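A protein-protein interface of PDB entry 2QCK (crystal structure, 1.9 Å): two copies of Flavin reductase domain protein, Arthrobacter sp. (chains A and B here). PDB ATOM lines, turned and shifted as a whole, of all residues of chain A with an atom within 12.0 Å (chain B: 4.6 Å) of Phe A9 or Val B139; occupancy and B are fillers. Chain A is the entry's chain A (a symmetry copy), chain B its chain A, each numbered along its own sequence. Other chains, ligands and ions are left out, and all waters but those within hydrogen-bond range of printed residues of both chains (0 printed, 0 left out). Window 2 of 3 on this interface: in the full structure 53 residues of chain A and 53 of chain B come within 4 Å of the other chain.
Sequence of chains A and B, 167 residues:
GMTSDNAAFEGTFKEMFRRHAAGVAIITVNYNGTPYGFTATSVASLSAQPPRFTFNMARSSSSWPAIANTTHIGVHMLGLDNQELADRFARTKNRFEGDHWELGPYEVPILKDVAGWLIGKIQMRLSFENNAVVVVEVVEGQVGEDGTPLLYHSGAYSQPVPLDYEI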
ATOM      1  N   PHE A   9     -10.033   6.967  14.581  1.00  0.00           N
ATOM      2  CA  PHE A   9     -10.955   8.002  14.008  1.00  0.00           C
ATOM      3  C   PHE A   9     -12.265   8.113  14.777  1.00  0.00           C
ATOM      4  O   PHE A   9     -12.741   9.210  15.057  1.00  0.00           O
ATOM      5  CB  PHE A   9     -11.273   7.716  12.541  1.00  0.00           C
ATOM      6  CG  PHE A   9     -12.270   8.689  11.935  1.00  0.00           C
ATOM      7  CD1 PHE A   9     -12.006  10.057  11.932  1.00  0.00           C
ATOM      8  CD2 PHE A   9     -13.460   8.233  11.367  1.00  0.00           C
ATOM      9  CE1 PHE A   9     -12.901  10.942  11.384  1.00  0.00           C
ATOM     10  CE2 PHE A   9     -14.360   9.117  10.807  1.00  0.00           C
ATOM     11  CZ  PHE A   9     -14.083  10.472  10.816  1.00  0.00           C
ATOM     12  N   GLU A  10     -12.869   6.969  15.073  1.00  0.00           N
ATOM     13  CA  GLU A  10     -13.863   6.887  16.139  1.00  0.00           C
ATOM     14  C   GLU A  10     -13.146   7.432  17.367  1.00  0.00           C
ATOM     15  O   GLU A  10     -13.735   8.147  18.185  1.00  0.00           O
ATOM     16  CB  GLU A  10     -14.303   5.433  16.380  1.00  0.00           C
ATOM     17  N   GLY A  11     -11.854   7.078  17.455  1.00  0.00           N
ATOM     18  CA  GLY A  11     -10.940   7.545  18.491  1.00  0.00           C
ATOM     19  C   GLY A  11     -10.662   9.025  18.437  1.00  0.00           C
ATOM     20  O   GLY A  11     -10.860   9.690  19.422  1.00  0.00           O
ATOM     21  N   THR A  12     -10.223   9.539  17.293  1.00  0.00           N
ATOM     22  CA  THR A  12      -9.900  10.970  17.153  1.00  0.00           C
ATOM     23  C   THR A  12     -11.080  11.865  17.552  1.00  0.00           C
ATOM     24  O   THR A  12     -10.913  12.795  18.338  1.00  0.00           O
ATOM     25  CB  THR A  12      -9.391  11.336  15.723  1.00  0.00           C
ATOM     26  OG1 THR A  12      -8.158  10.661  15.465  1.00  0.00           O
ATOM     27  CG2 THR A  12      -9.124  12.823  15.576  1.00  0.00           C
ATOM     28  N   PHE A  13     -12.270  11.580  17.030  1.00  0.00           N
ATOM     29  CA  PHE A  13     -13.477  12.315  17.417  1.00  0.00           C
ATOM     30  C   PHE A  13     -13.737  12.193  18.942  1.00  0.00           C
ATOM     31  O   PHE A  13     -13.915  13.201  19.629  1.00  0.00           O
ATOM     32  CB  PHE A  13     -14.676  11.831  16.573  1.00  0.00           C
ATOM     33  CG  PHE A  13     -15.983  12.437  16.957  1.00  0.00           C
ATOM     34  CD1 PHE A  13     -16.353  13.685  16.500  1.00  0.00           C
ATOM     35  CD2 PHE A  13     -16.867  11.747  17.776  1.00  0.00           C
ATOM     36  CE1 PHE A  13     -17.582  14.247  16.878  1.00  0.00           C
ATOM     37  CE2 PHE A  13     -18.084  12.308  18.141  1.00  0.00           C
ATOM     38  CZ  PHE A  13     -18.427  13.560  17.691  1.00  0.00           C
ATOM     39  N   LYS A  14     -13.736  10.988  19.498  1.00  0.00           N
ATOM     40  CA  LYS A  14     -13.990  10.852  20.956  1.00  0.00           C
ATOM     41  C   LYS A  14     -12.906  11.591  21.762  1.00  0.00           C
ATOM     42  O   LYS A  14     -13.192  12.239  22.769  1.00  0.00           O
ATOM     43  CB  LYS A  14     -14.083   9.383  21.416  1.00  0.00           C
ATOM     44  CG  LYS A  14     -15.530   8.883  21.697  1.00  0.00           C
ATOM     45  N   GLU A  15     -11.668  11.487  21.299  1.00  0.00           N
ATOM     46  CA  GLU A  15     -10.547  12.181  21.919  1.00  0.00           C
ATOM     47  C   GLU A  15     -10.716  13.697  21.889  1.00  0.00           C
ATOM     48  O   GLU A  15     -10.638  14.323  22.914  1.00  0.00           O
ATOM     49  CB  GLU A  15      -9.230  11.760  21.220  1.00  0.00           C
ATOM     50  CG  GLU A  15      -7.911  12.388  21.713  1.00  0.00           C
ATOM     51  CD  GLU A  15      -7.673  12.241  23.225  1.00  0.00           C
ATOM     52  OE1 GLU A  15      -8.443  11.527  23.931  1.00  0.00           O
ATOM     53  OE2 GLU A  15      -6.716  12.889  23.703  1.00  0.00           O
ATOM     54  N   MET A  16     -10.957  14.282  20.718  1.00  0.00           N
ATOM     55  CA  MET A  16     -11.080  15.737  20.618  1.00  0.00           C
ATOM     56  C   MET A  16     -12.175  16.277  21.541  1.00  0.00           C
ATOM     57  O   MET A  16     -12.002  17.352  22.103  1.00  0.00           O
ATOM     58  CB  MET A  16     -11.289  16.212  19.171  1.00  0.00           C
ATOM     59  CG  MET A  16     -10.091  16.134  18.255  1.00  0.00           C
ATOM     60  SD  MET A  16      -8.360  16.512  19.183  1.00  0.00           S
ATOM     61  CE  MET A  16      -8.848  18.343  19.830  1.00  0.00           C
ATOM     62  N   PHE A  17     -13.282  15.560  21.733  1.00  0.00           N
ATOM     63  CA  PHE A  17     -14.316  16.025  22.686  1.00  0.00           C
ATOM     64  C   PHE A  17     -13.978  15.739  24.143  1.00  0.00           C
ATOM     65  O   PHE A  17     -14.562  16.366  25.044  1.00  0.00           O
ATOM     66  CB  PHE A  17     -15.773  15.571  22.326  1.00  0.00           C
ATOM     67  CG  PHE A  17     -16.377  16.426  21.288  1.00  0.00           C
ATOM     68  CD1 PHE A  17     -16.877  17.665  21.619  1.00  0.00           C
ATOM     69  CD2 PHE A  17     -16.289  16.071  19.954  1.00  0.00           C
ATOM     70  CE1 PHE A  17     -17.328  18.510  20.649  1.00  0.00           C
ATOM     71  CE2 PHE A  17     -16.746  16.910  18.966  1.00  0.00           C
ATOM     72  CZ  PHE A  17     -17.262  18.130  19.316  1.00  0.00           C
ATOM     73  N   ARG A  18     -13.068  14.785  24.374  1.00  0.00           N
ATOM     74  CA  ARG A  18     -12.425  14.646  25.690  1.00  0.00           C
ATOM     75  C   ARG A  18     -11.635  15.898  26.030  1.00  0.00           C
ATOM     76  O   ARG A  18     -11.547  16.289  27.169  1.00  0.00           O
ATOM     77  CB  ARG A  18     -11.475  13.442  25.709  1.00  0.00           C
ATOM     78  CG  ARG A  18     -10.973  13.054  27.106  1.00  0.00           C
ATOM     79  CD  ARG A  18      -9.809  12.031  27.122  1.00  0.00           C
ATOM     80  NE  ARG A  18      -8.589  12.527  26.472  1.00  0.00           N
ATOM     81  CZ  ARG A  18      -7.785  13.460  26.983  1.00  0.00           C
ATOM     82  NH1 ARG A  18      -8.016  14.001  28.176  1.00  0.00           N
ATOM     83  NH2 ARG A  18      -6.719  13.853  26.301  1.00  0.00           N
ATOM     84  N   PRO B  51     -20.110  10.241  13.589  1.00  0.00           N
ATOM     85  CA  PRO B  51     -19.692  11.325  14.420  1.00  0.00           C
ATOM     86  C   PRO B  51     -20.248  12.633  13.930  1.00  0.00           C
ATOM     87  O   PRO B  51     -20.043  12.987  12.767  1.00  0.00           O
ATOM     88  CB  PRO B  51     -18.167  11.294  14.292  1.00  0.00           C
ATOM     89  CG  PRO B  51     -17.875  10.586  13.032  1.00  0.00           C
ATOM     90  CD  PRO B  51     -18.994   9.649  12.813  1.00  0.00           C
ATOM     91  N   TYR B 106      -9.971  19.137   1.835  1.00  0.00           N
ATOM     92  CA  TYR B 106     -11.096  19.851   1.254  1.00  0.00           C
ATOM     93  C   TYR B 106     -10.891  21.366   1.217  1.00  0.00           C
ATOM     94  O   TYR B 106     -11.867  22.129   1.135  1.00  0.00           O
ATOM     95  CB  TYR B 106     -12.378  19.505   1.999  1.00  0.00           C
ATOM     96  CG  TYR B 106     -12.582  18.023   2.226  1.00  0.00           C
ATOM     97  CD1 TYR B 106     -13.260  17.240   1.301  1.00  0.00           C
ATOM     98  CD2 TYR B 106     -12.108  17.409   3.361  1.00  0.00           C
ATOM     99  CE1 TYR B 106     -13.460  15.887   1.511  1.00  0.00           C
ATOM    100  CE2 TYR B 106     -12.307  16.060   3.588  1.00  0.00           C
ATOM    101  CZ  TYR B 106     -12.982  15.301   2.661  1.00  0.00           C
ATOM    102  OH  TYR B 106     -13.158  13.948   2.885  1.00  0.00           O
ATOM    103  N   ILE B 119     -12.532  17.883  10.663  1.00  0.00           N
ATOM    104  CA  ILE B 119     -13.150  18.415   9.445  1.00  0.00           C
ATOM    105  C   ILE B 119     -14.505  17.722   9.251  1.00  0.00           C
ATOM    106  O   ILE B 119     -14.650  16.508   9.416  1.00  0.00           O
ATOM    107  CB  ILE B 119     -12.228  18.272   8.188  1.00  0.00           C
ATOM    108  CG1 ILE B 119     -11.083  19.292   8.281  1.00  0.00           C
ATOM    109  CG2 ILE B 119     -12.996  18.507   6.867  1.00  0.00           C
ATOM    110  CD1 ILE B 119     -10.079  19.237   7.173  1.00  0.00           C
ATOM    111  N   GLY B 120     -15.514  18.516   8.917  1.00  0.00           N
ATOM    112  CA  GLY B 120     -16.852  17.990   8.753  1.00  0.00           C
ATOM    113  C   GLY B 120     -17.543  18.537   7.532  1.00  0.00           C
ATOM    114  O   GLY B 120     -17.077  19.514   6.922  1.00  0.00           O
ATOM    115  N   LYS B 121     -18.620  17.854   7.157  1.00  0.00           N
ATOM    116  CA  LYS B 121     -19.553  18.316   6.146  1.00  0.00           C
ATOM    117  C   LYS B 121     -20.767  18.813   6.874  1.00  0.00           C
ATOM    118  O   LYS B 121     -21.388  18.075   7.653  1.00  0.00           O
ATOM    119  CB  LYS B 121     -19.954  17.181   5.208  1.00  0.00           C
ATOM    120  CG  LYS B 121     -18.814  16.631   4.360  1.00  0.00           C
ATOM    121  N   GLU B 137     -21.345  16.616  10.118  1.00  0.00           N
ATOM    122  CA  GLU B 137     -20.854  15.244  10.210  1.00  0.00           C
ATOM    123  C   GLU B 137     -19.341  15.234   9.960  1.00  0.00           C
ATOM    124  O   GLU B 137     -18.867  15.740   8.932  1.00  0.00           O
ATOM    125  CB  GLU B 137     -21.541  14.349   9.168  1.00  0.00           C
ATOM    126  CG  GLU B 137     -21.094  12.868   9.297  1.00  0.00           C
ATOM    127  CD  GLU B 137     -21.811  11.890   8.376  1.00  0.00           C
ATOM    128  OE1 GLU B 137     -23.017  12.051   8.134  1.00  0.00           O
ATOM    129  OE2 GLU B 137     -21.183  10.902   7.957  1.00  0.00           O
ATOM    130  N   VAL B 138     -18.604  14.578  10.854  1.00  0.00           N
ATOM    131  CA  VAL B 138     -17.159  14.655  10.885  1.00  0.00           C
ATOM    132  C   VAL B 138     -16.624  13.629   9.900  1.00  0.00           C
ATOM    133  O   VAL B 138     -17.067  12.508   9.900  1.00  0.00           O
ATOM    134  CB  VAL B 138     -16.629  14.388  12.313  1.00  0.00           C
ATOM    135  CG1 VAL B 138     -15.123  14.248  12.355  1.00  0.00           C
ATOM    136  CG2 VAL B 138     -17.060  15.499  13.224  1.00  0.00           C
ATOM    137  N   VAL B 139     -15.720  14.053   9.032  1.00  0.00           N
ATOM    138  CA  VAL B 139     -15.130  13.163   8.024  1.00  0.00           C
ATOM    139  C   VAL B 139     -13.622  12.985   8.182  1.00  0.00           C
ATOM    140  O   VAL B 139     -13.025  12.071   7.574  1.00  0.00           O
ATOM    141  CB  VAL B 139     -15.450  13.628   6.585  1.00  0.00           C
ATOM    142  CG1 VAL B 139     -16.942  13.528   6.330  1.00  0.00           C
ATOM    143  CG2 VAL B 139     -14.926  15.061   6.311  1.00  0.00           C
ATOM    144  N   GLU B 140     -12.988  13.812   8.998  1.00  0.00           N
ATOM    145  CA  GLU B 140     -11.531  13.755   9.131  1.00  0.00           C
ATOM    146  C   GLU B 140     -11.141  14.459  10.411  1.00  0.00           C
ATOM    147  O   GLU B 140     -11.919  15.247  10.949  1.00  0.00           O
ATOM    148  CB  GLU B 140     -10.860  14.422   7.901  1.00  0.00           C
ATOM    149  CG  GLU B 140      -9.353  14.212   7.771  1.00  0.00           C
ATOM    150  CD  GLU B 140      -9.007  12.746   7.706  1.00  0.00           C
ATOM    151  OE1 GLU B 140      -9.097  12.187   6.581  1.00  0.00           O
ATOM    152  OE2 GLU B 140      -8.675  12.156   8.777  1.00  0.00           O
ATOM    153  N   GLY B 141      -9.945  14.183  10.913  1.00  0.00           N
ATOM    154  CA  GLY B 141      -9.458  14.902  12.096  1.00  0.00           C
ATOM    155  C   GLY B 141      -8.078  14.480  12.528  1.00  0.00           C
ATOM    156  O   GLY B 141      -7.501  13.569  11.953  1.00  0.00           O
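The backbone carbonyl oxygen of Pro B51 lies within hydrogen-bond range of the backbone NH of Val B138.
O of Ile B119 is in hydrogen-bond range of N of Val B139 (2.7 Å).
N of Ile B119 lies within hydrogen-bond range of O of Glu B140 (2.7 Å).
Among the printed residues, merely in contact across the chains: Phe A9 with Val B138 (3.7 Å), Phe A9 with Val B139 (3.7 Å), Phe A9 with Glu B140 (3.7 Å), Thr A12 with Gly B141 (3.6 Å), Phe A13 with Pro B51 (3.6 Å) and Phe A13 with Val B138 (3.8 Å).
Of the printed residues of chain B, Thr A12 touches Gly B141 (3.6 Å).
Printed residues of chain B within 4 Å of Phe A13: Pro B51 (3.6 Å) and Val B138 (3.8 Å).
Of chain A, only Phe A13 comes within 4 Å of Pro B51.
No residue of chain A comes within 4 Å of Gly B120.
Of the printed residues of chain A, Val B138 touches Phe A9 (3.7 Å) and Phe A13 (3.8 Å).
Val B139 touches one residue of chain A.
Of chain A, only Phe A9 (3.7 Å) comes within 4 Å of Glu B140.
Gly B141 touches just one residue of chain A: Thr A12.
The nearest residue of chain A that does not touch Val B139 is Phe A13 (7.5 Å).
The nearest printed residue of chain B that does not touch Thr A12 is Glu B140 (5.8 Å).
Of the 10 printed residues of chain B, 5 touch a printed residue of chain A.
Hydrophobic or aromatic side chains of chain B that line the printed part of chain A: Pro B51 and Val B138.
Along chain B the printed residues that touch a printed residue of chain A span positions 51 to 141.
Among the printed residues, no Asp or Glu carboxylate lies within 4 Å of a Lys or Arg side-chain nitrogen of the other chain.
No position is printed for both chains.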
